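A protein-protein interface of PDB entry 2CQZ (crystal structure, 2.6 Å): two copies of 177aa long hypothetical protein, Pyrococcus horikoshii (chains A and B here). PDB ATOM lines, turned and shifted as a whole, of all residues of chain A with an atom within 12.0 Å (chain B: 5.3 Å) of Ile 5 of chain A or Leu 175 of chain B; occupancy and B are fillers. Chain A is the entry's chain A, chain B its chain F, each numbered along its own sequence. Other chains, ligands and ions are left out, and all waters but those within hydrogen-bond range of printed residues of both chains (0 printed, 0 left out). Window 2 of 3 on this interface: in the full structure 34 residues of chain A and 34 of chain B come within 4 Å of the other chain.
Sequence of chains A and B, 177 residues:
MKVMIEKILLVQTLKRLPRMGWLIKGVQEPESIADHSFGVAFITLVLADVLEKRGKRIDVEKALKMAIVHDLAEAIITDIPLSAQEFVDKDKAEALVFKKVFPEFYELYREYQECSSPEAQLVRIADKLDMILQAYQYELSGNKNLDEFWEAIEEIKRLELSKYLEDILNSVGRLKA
No position is printed for both chains.
Ile 5 of chain A touches just these residues of chain B: Ile 168, Val 172 and Leu 175.
Leu 175 of chain B touches one residue of chain A.
Leu 133 of chain B touches just these residues of chain A: Ile 8 (3.6 Å), Leu 9 (3.9 Å) and Gln 12 (3.6 Å).
No residue of chain A comes within 4 Å of Tyr 136 of chain B.
Of the printed residues of chain A, Ile 168 of chain B touches Ile 5 (3.5 Å).
Val 172 of chain B touches just one residue of chain A: Ile 5.
No residue of chain A comes within 4 Å of Gly 173 of chain B.
Of the printed residues of chain B, Leu 9 of chain A touches Leu 133 (3.9 Å).
Of the printed residues of chain B, Ile 8 of chain A touches Leu 133 (3.6 Å).
Of the printed residues of chain B, Gln 12 of chain A touches Leu 133 (3.6 Å).
The nearest residue of chain A that does not touch Leu 175 of chain B is Leu 9 of chain A (4.4 Å).
Hydrophobic or aromatic side chains of chain B within 4 Å of the printed part of chain A: Leu 133, Ile 168, Val 172 and Leu 175.
Of the 18 printed residues of chain A, 4 touch a printed residue of chain B.
Hydrophobic or aromatic side chains of chain A that line the printed part of chain B: Ile 5, Ile 8 and Leu 9.
Along chain A the printed residues that touch a printed residue of chain B span positions 5 to 12.
Among the printed residues, pairs that only touch across the chains: Ile 5 of chain A with Val 172 of chain B (3.5 Å), Ile 5 of chain A with Ile 168 of chain B (3.5 Å), Gln 12 of chain A with Leu 133 of chain B (3.6 Å), Ile 5 of chain A with Leu 175 of chain B (3.6 Å), Ile 8 of chain A with Leu 133 of chain B (3.6 Å) and Leu 9 of chain A with Leu 133 of chain B (3.9 Å).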
ATOM      1  N   MET A   4      -0.324  15.976 -23.551  1.00  0.00           N
ATOM      2  CA  MET A   4      -0.167  17.070 -24.556  1.00  0.00           C
ATOM      3  C   MET A   4       1.239  17.031 -25.156  1.00  0.00           C
ATOM      4  O   MET A   4       2.224  16.761 -24.460  1.00  0.00           O
ATOM      5  CB  MET A   4      -0.377  18.442 -23.916  1.00  0.00           C
ATOM      6  CG  MET A   4       0.885  18.952 -23.248  1.00  0.00           C
ATOM      7  SD  MET A   4       0.802  20.579 -22.506  1.00  0.00           S
ATOM      8  CE  MET A   4       0.027  20.173 -20.878  1.00  0.00           C
ATOM      9  N   ILE A   5       1.318  17.330 -26.448  1.00  0.00           N
ATOM     10  CA  ILE A   5       2.570  17.326 -27.183  1.00  0.00           C
ATOM     11  C   ILE A   5       3.595  18.333 -26.675  1.00  0.00           C
ATOM     12  O   ILE A   5       4.784  18.030 -26.603  1.00  0.00           O
ATOM     13  CB  ILE A   5       2.287  17.558 -28.681  1.00  0.00           C
ATOM     14  CG1 ILE A   5       1.847  16.243 -29.312  1.00  0.00           C
ATOM     15  CG2 ILE A   5       3.511  18.111 -29.386  1.00  0.00           C
ATOM     16  CD1 ILE A   5       0.703  15.569 -28.593  1.00  0.00           C
ATOM     17  N   GLU A   6       3.137  19.524 -26.316  1.00  0.00           N
ATOM     18  CA  GLU A   6       4.034  20.560 -25.825  1.00  0.00           C
ATOM     19  C   GLU A   6       4.782  20.129 -24.555  1.00  0.00           C
ATOM     20  O   GLU A   6       5.970  20.428 -24.392  1.00  0.00           O
ATOM     21  CB  GLU A   6       3.245  21.844 -25.563  1.00  0.00           C
ATOM     22  CG  GLU A   6       4.117  23.070 -25.351  1.00  0.00           C
ATOM     23  CD  GLU A   6       3.307  24.342 -25.189  1.00  0.00           C
ATOM     24  OE1 GLU A   6       2.548  24.685 -26.126  1.00  0.00           O
ATOM     25  OE2 GLU A   6       3.427  24.998 -24.130  1.00  0.00           O
ATOM     26  N   LYS A   7       4.082  19.433 -23.664  1.00  0.00           N
ATOM     27  CA  LYS A   7       4.666  18.957 -22.414  1.00  0.00           C
ATOM     28  C   LYS A   7       5.747  17.922 -22.704  1.00  0.00           C
ATOM     29  O   LYS A   7       6.860  17.996 -22.176  1.00  0.00           O
ATOM     30  CB  LYS A   7       3.588  18.312 -21.541  1.00  0.00           C
ATOM     31  CG  LYS A   7       4.070  17.860 -20.183  1.00  0.00           C
ATOM     32  CD  LYS A   7       3.996  18.979 -19.163  1.00  0.00           C
ATOM     33  CE  LYS A   7       2.549  19.279 -18.807  1.00  0.00           C
ATOM     34  NZ  LYS A   7       2.411  20.169 -17.628  1.00  0.00           N
ATOM     35  N   ILE A   8       5.407  16.946 -23.539  1.00  0.00           N
ATOM     36  CA  ILE A   8       6.349  15.894 -23.894  1.00  0.00           C
ATOM     37  C   ILE A   8       7.596  16.458 -24.587  1.00  0.00           C
ATOM     38  O   ILE A   8       8.715  16.047 -24.301  1.00  0.00           O
ATOM     39  CB  ILE A   8       5.672  14.845 -24.799  1.00  0.00           C
ATOM     40  CG1 ILE A   8       4.491  14.217 -24.055  1.00  0.00           C
ATOM     41  CG2 ILE A   8       6.677  13.783 -25.195  1.00  0.00           C
ATOM     42  CD1 ILE A   8       3.669  13.282 -24.877  1.00  0.00           C
ATOM     43  N   LEU A   9       7.404  17.417 -25.481  1.00  0.00           N
ATOM     44  CA  LEU A   9       8.525  18.017 -26.191  1.00  0.00           C
ATOM     45  C   LEU A   9       9.429  18.761 -25.215  1.00  0.00           C
ATOM     46  O   LEU A   9      10.642  18.837 -25.397  1.00  0.00           O
ATOM     47  CB  LEU A   9       8.017  18.985 -27.262  1.00  0.00           C
ATOM     48  CG  LEU A   9       7.337  18.402 -28.508  1.00  0.00           C
ATOM     49  CD1 LEU A   9       6.831  19.552 -29.380  1.00  0.00           C
ATOM     50  CD2 LEU A   9       8.324  17.527 -29.285  1.00  0.00           C
ATOM     51  N   LEU A  10       8.818  19.318 -24.181  1.00  0.00           N
ATOM     52  CA  LEU A  10       9.545  20.045 -23.154  1.00  0.00           C
ATOM     53  C   LEU A  10      10.416  19.077 -22.344  1.00  0.00           C
ATOM     54  O   LEU A  10      11.601  19.362 -22.115  1.00  0.00           O
ATOM     55  CB  LEU A  10       8.572  20.741 -22.202  1.00  0.00           C
ATOM     56  CG  LEU A  10       9.273  21.351 -20.991  1.00  0.00           C
ATOM     57  CD1 LEU A  10      10.327  22.328 -21.460  1.00  0.00           C
ATOM     58  CD2 LEU A  10       8.265  22.033 -20.091  1.00  0.00           C
ATOM     59  N   VAL A  11       9.832  17.957 -21.898  1.00  0.00           N
ATOM     60  CA  VAL A  11      10.573  16.972 -21.100  1.00  0.00           C
ATOM     61  C   VAL A  11      11.638  16.240 -21.908  1.00  0.00           C
ATOM     62  O   VAL A  11      12.621  15.764 -21.342  1.00  0.00           O
ATOM     63  CB  VAL A  11       9.607  15.933 -20.429  1.00  0.00           C
ATOM     64  CG1 VAL A  11      10.358  14.640 -20.034  1.00  0.00           C
ATOM     65  CG2 VAL A  11       8.989  16.515 -19.165  1.00  0.00           C
ATOM     66  N   GLN A  12      11.450  16.165 -23.224  1.00  0.00           N
ATOM     67  CA  GLN A  12      12.438  15.519 -24.063  1.00  0.00           C
ATOM     68  C   GLN A  12      13.720  16.335 -24.117  1.00  0.00           C
ATOM     69  O   GLN A  12      14.735  15.860 -24.619  1.00  0.00           O
ATOM     70  CB  GLN A  12      11.911  15.304 -25.482  1.00  0.00           C
ATOM     71  CG  GLN A  12      10.902  14.158 -25.600  1.00  0.00           C
ATOM     72  CD  GLN A  12      10.757  13.629 -27.017  1.00  0.00           C
ATOM     73  OE1 GLN A  12      10.700  14.395 -27.983  1.00  0.00           O
ATOM     74  NE2 GLN A  12      10.681  12.312 -27.144  1.00  0.00           N
ATOM     75  N   THR A  13      13.676  17.564 -23.607  1.00  0.00           N
ATOM     76  CA  THR A  13      14.863  18.422 -23.579  1.00  0.00           C
ATOM     77  C   THR A  13      15.915  17.764 -22.675  1.00  0.00           C
ATOM     78  O   THR A  13      17.107  18.051 -22.773  1.00  0.00           O
ATOM     79  CB  THR A  13      14.533  19.821 -23.018  1.00  0.00           C
ATOM     80  OG1 THR A  13      13.406  20.355 -23.713  1.00  0.00           O
ATOM     81  CG2 THR A  13      15.698  20.772 -23.211  1.00  0.00           C
ATOM     82  N   LEU A  14      15.457  16.878 -21.795  1.00  0.00           N
ATOM     83  CA  LEU A  14      16.348  16.161 -20.892  1.00  0.00           C
ATOM     84  C   LEU A  14      17.324  15.266 -21.656  1.00  0.00           C
ATOM     85  O   LEU A  14      18.385  14.908 -21.133  1.00  0.00           O
ATOM     86  CB  LEU A  14      15.545  15.311 -19.898  1.00  0.00           C
ATOM     87  CG  LEU A  14      14.691  16.099 -18.893  1.00  0.00           C
ATOM     88  CD1 LEU A  14      13.982  15.123 -17.965  1.00  0.00           C
ATOM     89  CD2 LEU A  14      15.570  17.075 -18.101  1.00  0.00           C
ATOM     90  N   LYS A  15      16.966  14.899 -22.886  1.00  0.00           N
ATOM     91  CA  LYS A  15      17.831  14.062 -23.709  1.00  0.00           C
ATOM     92  C   LYS A  15      19.019  14.890 -24.148  1.00  0.00           C
ATOM     93  O   LYS A  15      20.092  14.351 -24.385  1.00  0.00           O
ATOM     94  CB  LYS A  15      17.097  13.563 -24.956  1.00  0.00           C
ATOM     95  CG  LYS A  15      15.936  12.639 -24.691  1.00  0.00           C
ATOM     96  CD  LYS A  15      15.318  12.144 -25.989  1.00  0.00           C
ATOM     97  CE  LYS A  15      14.247  11.117 -25.702  1.00  0.00           C
ATOM     98  NZ  LYS A  15      13.732  10.462 -26.924  1.00  0.00           N
ATOM     99  N   ARG A  16      18.829  16.204 -24.241  1.00  0.00           N
ATOM    100  CA  ARG A  16      19.897  17.096 -24.688  1.00  0.00           C
ATOM    101  C   ARG A  16      20.712  17.737 -23.592  1.00  0.00           C
ATOM    102  O   ARG A  16      21.831  18.177 -23.834  1.00  0.00           O
ATOM    103  CB  ARG A  16      19.336  18.224 -25.550  1.00  0.00           C
ATOM    104  CG  ARG A  16      18.576  17.764 -26.755  1.00  0.00           C
ATOM    105  CD  ARG A  16      18.347  18.913 -27.712  1.00  0.00           C
ATOM    106  NE  ARG A  16      17.371  19.885 -27.232  1.00  0.00           N
ATOM    107  CZ  ARG A  16      16.061  19.655 -27.152  1.00  0.00           C
ATOM    108  NH1 ARG A  16      15.566  18.475 -27.519  1.00  0.00           N
ATOM    109  NH2 ARG A  16      15.242  20.613 -26.714  1.00  0.00           N
ATOM    110  N   ALA A  75      14.205  20.124 -16.901  1.00  0.00           N
ATOM    111  CA  ALA A  75      13.885  20.322 -18.316  1.00  0.00           C
ATOM    112  C   ALA A  75      13.868  21.819 -18.630  1.00  0.00           C
ATOM    113  O   ALA A  75      14.040  22.237 -19.780  1.00  0.00           O
ATOM    114  CB  ALA A  75      12.531  19.700 -18.649  1.00  0.00           C
ATOM    115  N   VAL A 101       4.539  24.759 -13.889  1.00  0.00           N
ATOM    116  CA  VAL A 101       4.614  23.925 -15.095  1.00  0.00           C
ATOM    117  C   VAL A 101       4.155  22.462 -15.001  1.00  0.00           C
ATOM    118  O   VAL A 101       3.569  21.926 -15.954  1.00  0.00           O
ATOM    119  CB  VAL A 101       6.064  23.925 -15.682  1.00  0.00           C
ATOM    120  CG1 VAL A 101       6.119  23.097 -16.956  1.00  0.00           C
ATOM    121  CG2 VAL A 101       6.520  25.365 -15.954  1.00  0.00           C
ATOM    122  N   PHE A 102       4.456  21.816 -13.874  1.00  0.00           N
ATOM    123  CA  PHE A 102       4.105  20.404 -13.633  1.00  0.00           C
ATOM    124  C   PHE A 102       3.248  20.225 -12.376  1.00  0.00           C
ATOM    125  O   PHE A 102       3.563  19.406 -11.511  1.00  0.00           O
ATOM    126  CB  PHE A 102       5.392  19.562 -13.481  1.00  0.00           C
ATOM    127  CG  PHE A 102       6.269  19.576 -14.701  1.00  0.00           C
ATOM    128  CD1 PHE A 102       5.839  18.990 -15.887  1.00  0.00           C
ATOM    129  CD2 PHE A 102       7.506  20.207 -14.677  1.00  0.00           C
ATOM    130  CE1 PHE A 102       6.603  19.066 -17.035  1.00  0.00           C
ATOM    131  CE2 PHE A 102       8.288  20.286 -15.836  1.00  0.00           C
ATOM    132  CZ  PHE A 102       7.833  19.704 -17.011  1.00  0.00           C
ATOM    133  N   GLU A 104       0.545  18.736 -11.890  1.00  0.00           N
ATOM    134  CA  GLU A 104       0.098  17.354 -11.759  1.00  0.00           C
ATOM    135  C   GLU A 104       1.153  16.480 -11.112  1.00  0.00           C
ATOM    136  O   GLU A 104       0.824  15.426 -10.582  1.00  0.00           O
ATOM    137  CB  GLU A 104      -0.262  16.731 -13.117  1.00  0.00           C
ATOM    138  CG  GLU A 104       0.910  16.594 -14.063  1.00  0.00           C
ATOM    139  CD  GLU A 104       1.257  17.908 -14.729  1.00  0.00           C
ATOM    140  OE1 GLU A 104       1.099  18.957 -14.071  1.00  0.00           O
ATOM    141  OE2 GLU A 104       1.689  17.897 -15.902  1.00  0.00           O
ATOM    142  N   PHE A 105       2.418  16.892 -11.155  1.00  0.00           N
ATOM    143  CA  PHE A 105       3.463  16.078 -10.541  1.00  0.00           C
ATOM    144  C   PHE A 105       4.017  16.695  -9.267  1.00  0.00           C
ATOM    145  O   PHE A 105       4.988  16.183  -8.708  1.00  0.00           O
ATOM    146  CB  PHE A 105       4.627  15.832 -11.515  1.00  0.00           C
ATOM    147  CG  PHE A 105       4.241  15.070 -12.756  1.00  0.00           C
ATOM    148  CD1 PHE A 105       3.550  13.863 -12.668  1.00  0.00           C
ATOM    149  CD2 PHE A 105       4.586  15.559 -14.018  1.00  0.00           C
ATOM    150  CE1 PHE A 105       3.209  13.153 -13.815  1.00  0.00           C
ATOM    151  CE2 PHE A 105       4.254  14.862 -15.168  1.00  0.00           C
ATOM    152  CZ  PHE A 105       3.563  13.652 -15.069  1.00  0.00           C
ATOM    153  N   LEU B 133       8.333  12.184 -32.363  1.00  0.00           N
ATOM    154  CA  LEU B 133       8.700  13.483 -31.811  1.00  0.00           C
ATOM    155  C   LEU B 133      10.221  13.688 -31.854  1.00  0.00           C
ATOM    156  O   LEU B 133      10.695  14.816 -31.999  1.00  0.00           O
ATOM    157  CB  LEU B 133       8.168  13.617 -30.379  1.00  0.00           C
ATOM    158  CG  LEU B 133       6.638  13.611 -30.240  1.00  0.00           C
ATOM    159  CD1 LEU B 133       6.234  13.577 -28.772  1.00  0.00           C
ATOM    160  CD2 LEU B 133       6.069  14.849 -30.926  1.00  0.00           C
ATOM    161  N   TYR B 136      10.954  14.693 -35.273  1.00  0.00           N
ATOM    162  CA  TYR B 136      10.535  16.078 -35.403  1.00  0.00           C
ATOM    163  C   TYR B 136      11.668  17.011 -34.982  1.00  0.00           C
ATOM    164  O   TYR B 136      12.024  17.939 -35.712  1.00  0.00           O
ATOM    165  CB  TYR B 136       9.300  16.316 -34.532  1.00  0.00           C
ATOM    166  CG  TYR B 136       8.919  17.771 -34.358  1.00  0.00           C
ATOM    167  CD1 TYR B 136       8.407  18.515 -35.421  1.00  0.00           C
ATOM    168  CD2 TYR B 136       9.110  18.414 -33.135  1.00  0.00           C
ATOM    169  CE1 TYR B 136       8.102  19.870 -35.268  1.00  0.00           C
ATOM    170  CE2 TYR B 136       8.809  19.761 -32.976  1.00  0.00           C
ATOM    171  CZ  TYR B 136       8.308  20.482 -34.045  1.00  0.00           C
ATOM    172  OH  TYR B 136       8.037  21.820 -33.884  1.00  0.00           O
ATOM    173  N   TRP B 150       7.549   9.398 -39.914  1.00  0.00           N
ATOM    174  CA  TRP B 150       6.217   9.898 -39.629  1.00  0.00           C
ATOM    175  C   TRP B 150       5.113   8.927 -39.997  1.00  0.00           C
ATOM    176  O   TRP B 150       3.951   9.157 -39.656  1.00  0.00           O
ATOM    177  CB  TRP B 150       5.983  11.231 -40.325  1.00  0.00           C
ATOM    178  CG  TRP B 150       6.767  12.323 -39.712  1.00  0.00           C
ATOM    179  CD1 TRP B 150       8.077  12.618 -39.940  1.00  0.00           C
ATOM    180  CD2 TRP B 150       6.318  13.229 -38.703  1.00  0.00           C
ATOM    181  NE1 TRP B 150       8.473  13.667 -39.142  1.00  0.00           N
ATOM    182  CE2 TRP B 150       7.406  14.073 -38.386  1.00  0.00           C
ATOM    183  CE3 TRP B 150       5.090  13.440 -38.067  1.00  0.00           C
ATOM    184  CZ2 TRP B 150       7.319  15.080 -37.415  1.00  0.00           C
ATOM    185  CZ3 TRP B 150       5.001  14.444 -37.104  1.00  0.00           C
ATOM    186  CH2 TRP B 150       6.105  15.265 -36.804  1.00  0.00           C
ATOM    187  N   ILE B 168      -4.875  13.505 -29.697  1.00  0.00           N
ATOM    188  CA  ILE B 168      -3.436  13.650 -29.475  1.00  0.00           C
ATOM    189  C   ILE B 168      -2.668  13.314 -30.745  1.00  0.00           C
ATOM    190  O   ILE B 168      -1.750  14.035 -31.136  1.00  0.00           O
ATOM    191  CB  ILE B 168      -2.967  12.733 -28.319  1.00  0.00           C
ATOM    192  CG1 ILE B 168      -3.639  13.172 -27.018  1.00  0.00           C
ATOM    193  CG2 ILE B 168      -1.464  12.802 -28.154  1.00  0.00           C
ATOM    194  CD1 ILE B 168      -3.432  12.212 -25.883  1.00  0.00           C
ATOM    195  N   SER B 171      -2.654  16.117 -33.075  1.00  0.00           N
ATOM    196  CA  SER B 171      -1.752  17.226 -32.757  1.00  0.00           C
ATOM    197  C   SER B 171      -0.343  16.866 -33.201  1.00  0.00           C
ATOM    198  O   SER B 171       0.426  17.721 -33.639  1.00  0.00           O
ATOM    199  CB  SER B 171      -1.746  17.517 -31.255  1.00  0.00           C
ATOM    200  OG  SER B 171      -3.051  17.771 -30.773  1.00  0.00           O
ATOM    201  N   VAL B 172      -0.007  15.590 -33.081  1.00  0.00           N
ATOM    202  CA  VAL B 172       1.308  15.130 -33.477  1.00  0.00           C
ATOM    203  C   VAL B 172       1.481  15.257 -34.982  1.00  0.00           C
ATOM    204  O   VAL B 172       2.411  15.909 -35.446  1.00  0.00           O
ATOM    205  CB  VAL B 172       1.528  13.670 -33.056  1.00  0.00           C
ATOM    206  CG1 VAL B 172       2.856  13.159 -33.604  1.00  0.00           C
ATOM    207  CG2 VAL B 172       1.509  13.579 -31.546  1.00  0.00           C
ATOM    208  N   GLY B 173       0.581  14.633 -35.737  1.00  0.00           N
ATOM    209  CA  GLY B 173       0.671  14.693 -37.186  1.00  0.00           C
ATOM    210  C   GLY B 173       0.694  16.132 -37.651  1.00  0.00           C
ATOM    211  O   GLY B 173       1.236  16.473 -38.698  1.00  0.00           O
ATOM    212  N   ARG B 174       0.108  16.988 -36.835  1.00  0.00           N
ATOM    213  CA  ARG B 174       0.023  18.408 -37.114  1.00  0.00           C
ATOM    214  C   ARG B 174       1.396  19.094 -37.083  1.00  0.00           C
ATOM    215  O   ARG B 174       1.574  20.163 -37.660  1.00  0.00           O
ATOM    216  CB  ARG B 174      -0.928  19.027 -36.088  1.00  0.00           C
ATOM    217  CG  ARG B 174      -1.203  20.495 -36.222  1.00  0.00           C
ATOM    218  CD  ARG B 174      -2.373  20.869 -35.315  1.00  0.00           C
ATOM    219  NE  ARG B 174      -3.560  20.053 -35.578  1.00  0.00           N
ATOM    220  CZ  ARG B 174      -4.480  19.747 -34.662  1.00  0.00           C
ATOM    221  NH1 ARG B 174      -4.350  20.185 -33.416  1.00  0.00           N
ATOM    222  NH2 ARG B 174      -5.531  19.001 -34.991  1.00  0.00           N
ATOM    223  N   LEU B 175       2.359  18.465 -36.421  1.00  0.00           N
ATOM    224  CA  LEU B 175       3.712  19.008 -36.297  1.00  0.00           C
ATOM    225  C   LEU B 175       4.546  18.864 -37.566  1.00  0.00           C
ATOM    226  O   LEU B 175       5.516  19.598 -37.768  1.00  0.00           O
ATOM    227  CB  LEU B 175       4.454  18.323 -35.147  1.00  0.00           C
ATOM    228  CG  LEU B 175       4.072  18.677 -33.711  1.00  0.00           C
ATOM    229  CD1 LEU B 175       4.735  17.696 -32.753  1.00  0.00           C
ATOM    230  CD2 LEU B 175       4.500  20.107 -33.409  1.00  0.00           C
ATOM    231  N   LYS B 176       4.177  17.916 -38.417  1.00  0.00           N
ATOM    232  CA  LYS B 176       4.919  17.702 -39.650  1.00  0.00           C
ATOM    233  C   LYS B 176       4.746  18.882 -40.612  1.00  0.00           C
ATOM    234  O   LYS B 176       3.788  19.664 -40.437  1.00  0.00           O
ATOM    235  CB  LYS B 176       4.448  16.407 -40.311  1.00  0.00           C
ATOM    236  CG  LYS B 176       5.351  15.915 -41.412  1.00  0.00           C
ATOM    237  CD  LYS B 176       4.901  14.554 -41.894  1.00  0.00           C
ATOM    238  CE  LYS B 176       5.763  14.059 -43.043  1.00  0.00           C
ATOM    239  NZ  LYS B 176       5.351  12.697 -43.494  1.00  0.00           N
